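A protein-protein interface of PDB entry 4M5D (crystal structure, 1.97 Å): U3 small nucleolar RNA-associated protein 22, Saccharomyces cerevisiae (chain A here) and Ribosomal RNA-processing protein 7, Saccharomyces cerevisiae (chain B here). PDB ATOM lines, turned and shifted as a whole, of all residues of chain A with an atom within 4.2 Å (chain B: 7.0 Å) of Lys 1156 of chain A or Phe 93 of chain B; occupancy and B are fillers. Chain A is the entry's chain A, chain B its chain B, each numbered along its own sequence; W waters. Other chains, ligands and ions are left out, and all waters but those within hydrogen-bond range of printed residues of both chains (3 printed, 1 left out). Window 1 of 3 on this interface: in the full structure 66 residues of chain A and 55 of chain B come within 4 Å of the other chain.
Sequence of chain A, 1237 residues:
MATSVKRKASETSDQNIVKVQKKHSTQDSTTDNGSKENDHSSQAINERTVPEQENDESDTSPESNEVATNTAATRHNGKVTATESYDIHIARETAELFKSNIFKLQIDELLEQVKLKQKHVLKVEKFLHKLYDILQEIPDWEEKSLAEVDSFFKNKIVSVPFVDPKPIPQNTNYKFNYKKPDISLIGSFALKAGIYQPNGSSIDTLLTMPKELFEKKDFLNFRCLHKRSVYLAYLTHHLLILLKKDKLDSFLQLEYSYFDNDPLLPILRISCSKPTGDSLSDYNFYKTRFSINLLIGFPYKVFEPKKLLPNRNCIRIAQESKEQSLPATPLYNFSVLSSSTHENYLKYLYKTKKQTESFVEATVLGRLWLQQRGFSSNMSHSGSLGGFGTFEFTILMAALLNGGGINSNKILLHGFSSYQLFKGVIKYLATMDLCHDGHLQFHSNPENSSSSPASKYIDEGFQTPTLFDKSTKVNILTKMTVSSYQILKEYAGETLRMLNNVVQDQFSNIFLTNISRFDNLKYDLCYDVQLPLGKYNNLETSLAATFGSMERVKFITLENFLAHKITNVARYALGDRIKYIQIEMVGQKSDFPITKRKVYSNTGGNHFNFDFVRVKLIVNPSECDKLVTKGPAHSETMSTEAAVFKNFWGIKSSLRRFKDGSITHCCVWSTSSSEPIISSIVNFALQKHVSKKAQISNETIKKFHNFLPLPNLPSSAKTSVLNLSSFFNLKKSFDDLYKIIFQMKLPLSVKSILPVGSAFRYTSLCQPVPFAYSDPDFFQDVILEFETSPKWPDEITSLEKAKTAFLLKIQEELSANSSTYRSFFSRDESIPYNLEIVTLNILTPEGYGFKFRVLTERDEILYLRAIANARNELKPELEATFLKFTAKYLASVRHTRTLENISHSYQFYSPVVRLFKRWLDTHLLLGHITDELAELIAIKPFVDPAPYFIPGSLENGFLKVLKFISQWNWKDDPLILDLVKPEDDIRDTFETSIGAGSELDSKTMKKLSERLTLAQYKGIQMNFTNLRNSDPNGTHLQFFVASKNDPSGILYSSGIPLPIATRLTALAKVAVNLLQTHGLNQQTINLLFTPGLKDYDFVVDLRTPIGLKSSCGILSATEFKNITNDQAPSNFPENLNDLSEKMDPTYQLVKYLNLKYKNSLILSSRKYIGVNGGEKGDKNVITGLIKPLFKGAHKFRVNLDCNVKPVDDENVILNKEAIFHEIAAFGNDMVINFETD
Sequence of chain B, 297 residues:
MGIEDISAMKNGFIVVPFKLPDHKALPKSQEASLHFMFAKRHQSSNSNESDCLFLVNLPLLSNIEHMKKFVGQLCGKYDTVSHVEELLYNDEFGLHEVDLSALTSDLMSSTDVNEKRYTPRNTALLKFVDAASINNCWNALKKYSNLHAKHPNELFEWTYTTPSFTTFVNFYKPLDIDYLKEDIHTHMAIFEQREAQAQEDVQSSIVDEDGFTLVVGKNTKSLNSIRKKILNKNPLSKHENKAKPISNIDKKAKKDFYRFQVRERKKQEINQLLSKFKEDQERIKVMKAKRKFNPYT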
ATOM      1  N   TYR A1152      -7.063  21.362 -24.375  1.00  0.00           N
ATOM      2  CA  TYR A1152      -8.375  21.957 -24.127  1.00  0.00           C
ATOM      3  C   TYR A1152      -8.385  22.942 -22.959  1.00  0.00           C
ATOM      4  O   TYR A1152      -9.109  23.938 -22.998  1.00  0.00           O
ATOM      5  CB  TYR A1152      -9.467  20.878 -24.017  1.00  0.00           C
ATOM      6  CG  TYR A1152      -9.783  20.317 -25.390  1.00  0.00           C
ATOM      7  CD1 TYR A1152     -10.517  21.067 -26.312  1.00  0.00           C
ATOM      8  CD2 TYR A1152      -9.303  19.067 -25.785  1.00  0.00           C
ATOM      9  CE1 TYR A1152     -10.786  20.586 -27.590  1.00  0.00           C
ATOM     10  CE2 TYR A1152      -9.565  18.571 -27.063  1.00  0.00           C
ATOM     11  CZ  TYR A1152     -10.303  19.336 -27.957  1.00  0.00           C
ATOM     12  OH  TYR A1152     -10.559  18.853 -29.218  1.00  0.00           O
ATOM     13  N   LEU A1153      -7.563  22.674 -21.951  1.00  0.00           N
ATOM     14  CA  LEU A1153      -7.359  23.654 -20.880  1.00  0.00           C
ATOM     15  C   LEU A1153      -6.821  24.979 -21.436  1.00  0.00           C
ATOM     16  O   LEU A1153      -7.296  26.055 -21.069  1.00  0.00           O
ATOM     17  CB  LEU A1153      -6.423  23.096 -19.814  1.00  0.00           C
ATOM     18  CG  LEU A1153      -6.966  22.037 -18.854  1.00  0.00           C
ATOM     19  CD1 LEU A1153      -5.820  21.472 -18.028  1.00  0.00           C
ATOM     20  CD2 LEU A1153      -8.060  22.615 -17.942  1.00  0.00           C
ATOM     21  N   ASN A1154      -5.832  24.908 -22.324  1.00  0.00           N
ATOM     22  CA  ASN A1154      -5.303  26.128 -22.927  1.00  0.00           C
ATOM     23  C   ASN A1154      -6.327  26.873 -23.774  1.00  0.00           C
ATOM     24  O   ASN A1154      -6.342  28.111 -23.795  1.00  0.00           O
ATOM     25  CB  ASN A1154      -4.021  25.846 -23.734  1.00  0.00           C
ATOM     26  CG  ASN A1154      -2.779  25.922 -22.878  1.00  0.00           C
ATOM     27  OD1 ASN A1154      -1.919  25.048 -22.942  1.00  0.00           O
ATOM     28  ND2 ASN A1154      -2.681  26.966 -22.057  1.00  0.00           N
ATOM     29  N   LEU A1155      -7.196  26.127 -24.451  1.00  0.00           N
ATOM     30  CA  LEU A1155      -8.244  26.731 -25.262  1.00  0.00           C
ATOM     31  C   LEU A1155      -9.288  27.417 -24.389  1.00  0.00           C
ATOM     32  O   LEU A1155      -9.763  28.499 -24.718  1.00  0.00           O
ATOM     33  CB  LEU A1155      -8.897  25.675 -26.151  1.00  0.00           C
ATOM     34  CG  LEU A1155      -8.053  25.195 -27.349  1.00  0.00           C
ATOM     35  CD1 LEU A1155      -8.786  24.102 -28.097  1.00  0.00           C
ATOM     36  CD2 LEU A1155      -7.701  26.360 -28.296  1.00  0.00           C
ATOM     37  N   LYS A1156      -9.634  26.787 -23.269  1.00  0.00           N
ATOM     38  CA  LYS A1156     -10.615  27.366 -22.362  1.00  0.00           C
ATOM     39  C   LYS A1156     -10.052  28.599 -21.650  1.00  0.00           C
ATOM     40  O   LYS A1156     -10.699  29.627 -21.605  1.00  0.00           O
ATOM     41  CB  LYS A1156     -11.093  26.341 -21.328  1.00  0.00           C
ATOM     42  CG  LYS A1156     -12.116  26.924 -20.322  1.00  0.00           C
ATOM     43  CD  LYS A1156     -12.586  25.854 -19.332  1.00  0.00           C
ATOM     44  CE  LYS A1156     -13.470  26.459 -18.232  1.00  0.00           C
ATOM     45  NZ  LYS A1156     -14.775  26.887 -18.758  1.00  0.00           N
ATOM     46  N   TYR A1157      -8.840  28.487 -21.113  1.00  0.00           N
ATOM     47  CA  TYR A1157      -8.298  29.529 -20.241  1.00  0.00           C
ATOM     48  C   TYR A1157      -7.295  30.472 -20.907  1.00  0.00           C
ATOM     49  O   TYR A1157      -6.551  31.164 -20.212  1.00  0.00           O
ATOM     50  CB  TYR A1157      -7.636  28.890 -19.030  1.00  0.00           C
ATOM     51  CG  TYR A1157      -8.586  28.114 -18.148  1.00  0.00           C
ATOM     52  CD1 TYR A1157      -9.490  28.780 -17.302  1.00  0.00           C
ATOM     53  CD2 TYR A1157      -8.572  26.721 -18.147  1.00  0.00           C
ATOM     54  CE1 TYR A1157     -10.360  28.067 -16.479  1.00  0.00           C
ATOM     55  CE2 TYR A1157      -9.431  26.000 -17.331  1.00  0.00           C
ATOM     56  CZ  TYR A1157     -10.321  26.679 -16.503  1.00  0.00           C
ATOM     57  OH  TYR A1157     -11.159  25.947 -15.705  1.00  0.00           O
ATOM     58  N   LYS A1158      -7.302  30.517 -22.236  1.00  0.00           N
ATOM     59  CA  LYS A1158      -6.297  31.283 -22.994  1.00  0.00           C
ATOM     60  C   LYS A1158      -6.191  32.722 -22.501  1.00  0.00           C
ATOM     61  O   LYS A1158      -5.091  33.249 -22.348  1.00  0.00           O
ATOM     62  CB  LYS A1158      -6.632  31.275 -24.484  1.00  0.00           C
ATOM     63  CG  LYS A1158      -5.402  31.187 -25.392  1.00  0.00           C
ATOM     64  CD  LYS A1158      -5.787  31.317 -26.876  1.00  0.00           C
ATOM     65  CE  LYS A1158      -6.345  30.015 -27.474  1.00  0.00           C
ATOM     66  NZ  LYS A1158      -5.299  29.196 -28.191  1.00  0.00           N
ATOM     67  N   GLU A1222     -11.951  23.252 -11.197  1.00  0.00           N
ATOM     68  CA  GLU A1222     -12.239  22.944 -12.599  1.00  0.00           C
ATOM     69  C   GLU A1222     -11.129  22.094 -13.219  1.00  0.00           C
ATOM     70  O   GLU A1222     -11.399  21.062 -13.859  1.00  0.00           O
ATOM     71  CB  GLU A1222     -12.475  24.218 -13.410  1.00  0.00           C
ATOM     72  CG  GLU A1222     -13.792  24.916 -13.080  1.00  0.00           C
ATOM     73  CD  GLU A1222     -14.072  26.136 -13.934  1.00  0.00           C
ATOM     74  OE1 GLU A1222     -13.122  26.883 -14.311  1.00  0.00           O
ATOM     75  OE2 GLU A1222     -15.266  26.373 -14.214  1.00  0.00           O
ATOM     76  N   HIS B  35     -18.203  28.511  -6.935  1.00  0.00           N
ATOM     77  CA  HIS B  35     -18.142  29.091  -8.271  1.00  0.00           C
ATOM     78  C   HIS B  35     -19.290  30.074  -8.429  1.00  0.00           C
ATOM     79  O   HIS B  35     -20.425  29.765  -8.038  1.00  0.00           O
ATOM     80  CB  HIS B  35     -18.281  27.998  -9.343  1.00  0.00           C
ATOM     81  CG  HIS B  35     -18.351  28.531 -10.741  1.00  0.00           C
ATOM     82  ND1 HIS B  35     -17.286  28.471 -11.615  1.00  0.00           N
ATOM     83  CD2 HIS B  35     -19.352  29.153 -11.411  1.00  0.00           C
ATOM     84  CE1 HIS B  35     -17.631  29.026 -12.764  1.00  0.00           C
ATOM     85  NE2 HIS B  35     -18.880  29.445 -12.667  1.00  0.00           N
ATOM     86  N   ASN B  57     -20.076  33.258 -17.133  1.00  0.00           N
ATOM     87  CA  ASN B  57     -19.222  32.407 -16.295  1.00  0.00           C
ATOM     88  C   ASN B  57     -19.874  31.078 -15.882  1.00  0.00           C
ATOM     89  O   ASN B  57     -20.069  30.782 -14.689  1.00  0.00           O
ATOM     90  CB  ASN B  57     -18.665  33.176 -15.086  1.00  0.00           C
ATOM     91  CG  ASN B  57     -17.504  32.464 -14.438  1.00  0.00           C
ATOM     92  OD1 ASN B  57     -16.722  31.772 -15.115  1.00  0.00           O
ATOM     93  ND2 ASN B  57     -17.375  32.615 -13.126  1.00  0.00           N
ATOM     94  N   LEU B  58     -20.215  30.281 -16.889  1.00  0.00           N
ATOM     95  CA  LEU B  58     -20.760  28.956 -16.663  1.00  0.00           C
ATOM     96  C   LEU B  58     -19.638  28.068 -16.153  1.00  0.00           C
ATOM     97  O   LEU B  58     -18.483  28.238 -16.546  1.00  0.00           O
ATOM     98  CB  LEU B  58     -21.375  28.377 -17.947  1.00  0.00           C
ATOM     99  CG  LEU B  58     -22.604  29.047 -18.580  1.00  0.00           C
ATOM    100  CD1 LEU B  58     -22.237  30.338 -19.283  1.00  0.00           C
ATOM    101  CD2 LEU B  58     -23.257  28.098 -19.575  1.00  0.00           C
ATOM    102  N   PRO B  59     -19.971  27.124 -15.258  1.00  0.00           N
ATOM    103  CA  PRO B  59     -19.005  26.168 -14.765  1.00  0.00           C
ATOM    104  C   PRO B  59     -18.452  25.292 -15.893  1.00  0.00           C
ATOM    105  O   PRO B  59     -19.119  25.089 -16.914  1.00  0.00           O
ATOM    106  CB  PRO B  59     -19.830  25.312 -13.795  1.00  0.00           C
ATOM    107  CG  PRO B  59     -20.998  26.174 -13.424  1.00  0.00           C
ATOM    108  CD  PRO B  59     -21.302  26.927 -14.660  1.00  0.00           C
ATOM    109  N   LEU B  60     -17.245  24.788 -15.685  1.00  0.00           N
ATOM    110  CA  LEU B  60     -16.591  23.872 -16.615  1.00  0.00           C
ATOM    111  C   LEU B  60     -17.567  22.862 -17.203  1.00  0.00           C
ATOM    112  O   LEU B  60     -18.319  22.209 -16.469  1.00  0.00           O
ATOM    113  CB  LEU B  60     -15.446  23.132 -15.910  1.00  0.00           C
ATOM    114  CG  LEU B  60     -14.737  22.006 -16.688  1.00  0.00           C
ATOM    115  CD1 LEU B  60     -13.774  22.574 -17.736  1.00  0.00           C
ATOM    116  CD2 LEU B  60     -14.019  21.056 -15.737  1.00  0.00           C
ATOM    117  N   LEU B  61     -17.552  22.744 -18.530  1.00  0.00           N
ATOM    118  CA  LEU B  61     -18.282  21.689 -19.245  1.00  0.00           C
ATOM    119  C   LEU B  61     -19.796  21.688 -19.019  1.00  0.00           C
ATOM    120  O   LEU B  61     -20.433  20.635 -19.013  1.00  0.00           O
ATOM    121  CB  LEU B  61     -17.676  20.307 -18.935  1.00  0.00           C
ATOM    122  CG  LEU B  61     -16.295  20.008 -19.532  1.00  0.00           C
ATOM    123  CD1 LEU B  61     -15.756  18.684 -19.011  1.00  0.00           C
ATOM    124  CD2 LEU B  61     -16.342  20.037 -21.071  1.00  0.00           C
ATOM    125  N   SER B  62     -20.366  22.876 -18.836  1.00  0.00           N
ATOM    126  CA  SER B  62     -21.811  23.036 -18.732  1.00  0.00           C
ATOM    127  C   SER B  62     -22.470  22.544 -20.008  1.00  0.00           C
ATOM    128  O   SER B  62     -21.976  22.801 -21.104  1.00  0.00           O
ATOM    129  CB  SER B  62     -22.184  24.505 -18.505  1.00  0.00           C
ATOM    130  OG  SER B  62     -21.915  24.885 -17.168  1.00  0.00           O
ATOM    131  N   ASN B  90     -22.937  28.137 -26.345  1.00  0.00           N
ATOM    132  CA  ASN B  90     -21.991  27.674 -25.348  1.00  0.00           C
ATOM    133  C   ASN B  90     -20.730  27.160 -26.043  1.00  0.00           C
ATOM    134  O   ASN B  90     -20.619  25.973 -26.341  1.00  0.00           O
ATOM    135  CB  ASN B  90     -22.628  26.595 -24.463  1.00  0.00           C
ATOM    136  CG  ASN B  90     -21.704  26.127 -23.351  1.00  0.00           C
ATOM    137  OD1 ASN B  90     -20.943  26.912 -22.784  1.00  0.00           O
ATOM    138  ND2 ASN B  90     -21.766  24.840 -23.036  1.00  0.00           N
ATOM    139  N   ASP B  91     -19.798  28.069 -26.317  1.00  0.00           N
ATOM    140  CA  ASP B  91     -18.556  27.732 -27.028  1.00  0.00           C
ATOM    141  C   ASP B  91     -17.365  27.871 -26.080  1.00  0.00           C
ATOM    142  O   ASP B  91     -16.509  28.742 -26.233  1.00  0.00           O
ATOM    143  CB  ASP B  91     -18.395  28.600 -28.284  1.00  0.00           C
ATOM    144  CG  ASP B  91     -17.221  28.155 -29.170  1.00  0.00           C
ATOM    145  OD1 ASP B  91     -16.702  27.026 -28.990  1.00  0.00           O
ATOM    146  OD2 ASP B  91     -16.822  28.955 -30.035  1.00  0.00           O
ATOM    147  N   GLU B  92     -17.349  26.982 -25.095  1.00  0.00           N
ATOM    148  CA  GLU B  92     -16.426  27.010 -23.967  1.00  0.00           C
ATOM    149  C   GLU B  92     -14.948  27.022 -24.381  1.00  0.00           C
ATOM    150  O   GLU B  92     -14.095  27.614 -23.700  1.00  0.00           O
ATOM    151  CB  GLU B  92     -16.722  25.789 -23.095  1.00  0.00           C
ATOM    152  CG  GLU B  92     -15.849  25.639 -21.893  1.00  0.00           C
ATOM    153  CD  GLU B  92     -16.335  24.554 -20.956  1.00  0.00           C
ATOM    154  OE1 GLU B  92     -17.150  23.704 -21.378  1.00  0.00           O
ATOM    155  OE2 GLU B  92     -15.890  24.564 -19.794  1.00  0.00           O
ATOM    156  N   PHE B  93     -14.647  26.383 -25.506  1.00  0.00           N
ATOM    157  CA  PHE B  93     -13.261  26.260 -25.950  1.00  0.00           C
ATOM    158  C   PHE B  93     -12.862  27.198 -27.097  1.00  0.00           C
ATOM    159  O   PHE B  93     -11.729  27.140 -27.599  1.00  0.00           O
ATOM    160  CB  PHE B  93     -12.931  24.790 -26.233  1.00  0.00           C
ATOM    161  CG  PHE B  93     -13.098  23.912 -25.028  1.00  0.00           C
ATOM    162  CD1 PHE B  93     -12.163  23.949 -23.992  1.00  0.00           C
ATOM    163  CD2 PHE B  93     -14.212  23.085 -24.900  1.00  0.00           C
ATOM    164  CE1 PHE B  93     -12.312  23.149 -22.855  1.00  0.00           C
ATOM    165  CE2 PHE B  93     -14.383  22.285 -23.766  1.00  0.00           C
ATOM    166  CZ  PHE B  93     -13.431  22.319 -22.733  1.00  0.00           C
ATOM    167  N   GLY B  94     -13.789  28.075 -27.477  1.00  0.00           N
ATOM    168  CA  GLY B  94     -13.523  29.143 -28.446  1.00  0.00           C
ATOM    169  C   GLY B  94     -13.404  28.655 -29.880  1.00  0.00           C
ATOM    170  O   GLY B  94     -12.906  29.371 -30.745  1.00  0.00           O
ATOM    171  N   LEU B  95     -13.871  27.436 -30.128  1.00  0.00           N
ATOM    172  CA  LEU B  95     -13.675  26.784 -31.424  1.00  0.00           C
ATOM    173  C   LEU B  95     -14.486  27.400 -32.571  1.00  0.00           C
ATOM    174  O   LEU B  95     -14.090  27.286 -33.728  1.00  0.00           O
ATOM    175  CB  LEU B  95     -13.943  25.283 -31.309  1.00  0.00           C
ATOM    176  CG  LEU B  95     -13.018  24.496 -30.367  1.00  0.00           C
ATOM    177  CD1 LEU B  95     -13.658  23.172 -29.970  1.00  0.00           C
ATOM    178  CD2 LEU B  95     -11.619  24.265 -30.978  1.00  0.00           C
ATOM    179  N   HIS B  96     -15.595  28.067 -32.249  1.00  0.00           N
ATOM    180  CA  HIS B  96     -16.496  28.638 -33.260  1.00  0.00           C
ATOM    181  C   HIS B  96     -16.569  30.163 -33.188  1.00  0.00           C
ATOM    182  O   HIS B  96     -17.480  30.773 -33.747  1.00  0.00           O
ATOM    183  CB  HIS B  96     -17.907  28.044 -33.117  1.00  0.00           C
ATOM    184  CG  HIS B  96     -17.930  26.549 -33.132  1.00  0.00           C
ATOM    185  ND1 HIS B  96     -17.710  25.789 -32.002  1.00  0.00           N
ATOM    186  CD2 HIS B  96     -18.121  25.670 -34.145  1.00  0.00           C
ATOM    187  CE1 HIS B  96     -17.773  24.506 -32.317  1.00  0.00           C
ATOM    188  NE2 HIS B  96     -18.020  24.408 -33.612  1.00  0.00           N
ATOM    189  N   GLU B  97     -15.597  30.770 -32.515  1.00  0.00           N
ATOM    190  CA  GLU B  97     -15.589  32.214 -32.245  1.00  0.00           C
ATOM    191  C   GLU B  97     -15.613  33.103 -33.502  1.00  0.00           C
ATOM    192  O   GLU B  97     -16.181  34.195 -33.497  1.00  0.00           O
ATOM    193  CB  GLU B  97     -14.385  32.564 -31.378  1.00  0.00           C
ATOM    194  CG  GLU B  97     -14.570  33.813 -30.543  1.00  0.00           C
ATOM    195  CD  GLU B  97     -13.422  34.052 -29.572  1.00  0.00           C
ATOM    196  OE1 GLU B  97     -12.881  33.065 -29.018  1.00  0.00           O
ATOM    197  OE2 GLU B  97     -13.072  35.235 -29.353  1.00  0.00           O
ATOM    198  N   ARG B 121     -17.496  35.663 -25.190  1.00  0.00           N
ATOM    199  CA  ARG B 121     -16.710  34.484 -24.833  1.00  0.00           C
ATOM    200  C   ARG B 121     -16.928  34.219 -23.338  1.00  0.00           C
ATOM    201  O   ARG B 121     -16.982  35.173 -22.546  1.00  0.00           O
ATOM    202  CB  ARG B 121     -15.235  34.728 -25.145  1.00  0.00           C
ATOM    203  CG  ARG B 121     -14.328  33.546 -24.915  1.00  0.00           C
ATOM    204  CD  ARG B 121     -13.180  33.563 -25.909  1.00  0.00           C
ATOM    205  NE  ARG B 121     -11.964  32.918 -25.408  1.00  0.00           N
ATOM    206  CZ  ARG B 121     -11.786  31.604 -25.265  1.00  0.00           C
ATOM    207  NH1 ARG B 121     -12.752  30.743 -25.546  1.00  0.00           N
ATOM    208  NH2 ARG B 121     -10.630  31.152 -24.804  1.00  0.00           N
ATOM    209  N   ASN B 122     -17.060  32.941 -22.961  1.00  0.00           N
ATOM    210  CA  ASN B 122     -17.379  32.525 -21.577  1.00  0.00           C
ATOM    211  C   ASN B 122     -18.856  32.761 -21.188  1.00  0.00           C
ATOM    212  O   ASN B 122     -19.210  32.776 -20.005  1.00  0.00           O
ATOM    213  CB  ASN B 122     -16.447  33.213 -20.558  1.00  0.00           C
ATOM    214  CG  ASN B 122     -16.454  32.533 -19.207  1.00  0.00           C
ATOM    215  OD1 ASN B 122     -16.605  31.321 -19.125  1.00  0.00           O
ATOM    216  ND2 ASN B 122     -16.290  33.311 -18.139  1.00  0.00           N
HETATM  217  O   HOH W   1     -16.680  25.838 -11.974  1.00  0.00           O
HETATM  218  O   HOH W   2     -15.814  27.725 -16.221  1.00  0.00           O
HETATM  219  O   HOH W   3     -10.154  32.076 -22.251  1.00  0.00           O
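Water W2 lies within hydrogen-bond range of OE2 of Glu 1222 of chain A, O of Leu 58 of chain B, NZ of Lys 1156 of chain A and N of Leu 60 of chain B. Water W3 lies within hydrogen-bond range of O of Lys 1156 of chain A, NH2 of Arg 121 of chain B and N of Lys 1158 of chain A. Water W1 bridges the side-chain carboxylate of Glu 1222 of chain A (2.7 Å) and a ring nitrogen (ND1) of His 35 of chain B (2.7 Å).
The backbone carbonyl oxygen (O) of Leu 1155 of chain A sits at hydrogen-bond distance from the guanidinium group (NH2) of Arg 121 of chain B (2.8 Å). The side-chain carboxylate of Glu 92 of chain B lies within salt-bridge range of the side-chain amino group of Lys 1156 of chain A, 2.8 Å away. OE2 of Glu 1222 of chain A lies within hydrogen-bond range of N of Leu 60 of chain B, at 2.9 Å.
O of Tyr 1152 of chain A touches CD1 of Phe 93 of chain B (3.2 Å). Leu 1155 of chain A touches Phe 93 of chain B (CB to O, 3.5 Å). Leu 60 of chain B touches Lys 1156 of chain A (CD1 to CD, 3.8 Å). CB of Lys 1156 of chain A touches CD1 of Phe 93 of chain B (3.7 Å). Arg 121 of chain B touches Lys 1156 of chain A. OE2 of Glu 1222 of chain A touches CE1 of His 35 of chain B, 3.8 Å away. Pro 59 of chain B touches Glu 1222 of chain A (C to OE2, 3.8 Å).
The side-chain carboxylate (OE1) of Glu 1222 of chain A is in hydrogen-bond range of the side-chain hydroxyl (OH) of Tyr 1157 of chain A (2.6 Å). A ring nitrogen (NE2) of His 35 of chain B sits at hydrogen-bond distance from the backbone carbonyl oxygen of Asn 57 of chain B (2.7 Å). O of Pro 59 of chain B sits at hydrogen-bond distance from OG of Ser 62 of chain B, 2.8 Å away. N of Leu 61 of chain B sits at hydrogen-bond distance from OE2 of Glu 92 of chain B (2.8 Å). OE1 of Glu 97 of chain B lies within salt-bridge range of NE of Arg 121 of chain B (3.7 Å).
Of the 8 printed residues of chain A, 4 touch a printed residue of chain B. Among the printed residues, Asp or Glu carboxylates within 4 Å of a Lys or Arg side-chain nitrogen of the other chain: Lys 1156 of chain A with Glu 92 of chain B (2.8 Å).
Of the printed residues of chain B, Tyr 1152 of chain A touches Phe 93. Of the printed residues of chain B, Leu 1155 of chain A touches Phe 93 and Arg 121. Of chain B, only Leu 60, Glu 92, Phe 93 and Arg 121 come within 4 Å of Lys 1156 of chain A. Of the printed residues of chain A, Pro 59 of chain B touches Glu 1222 (3.8 Å). Phe 93 of chain B touches three residues of chain A. His 96 of chain B touches none of the printed residues of chain A. Printed residues of chain A within 4 Å of Arg 121 of chain B: Leu 1155 and Lys 1156.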
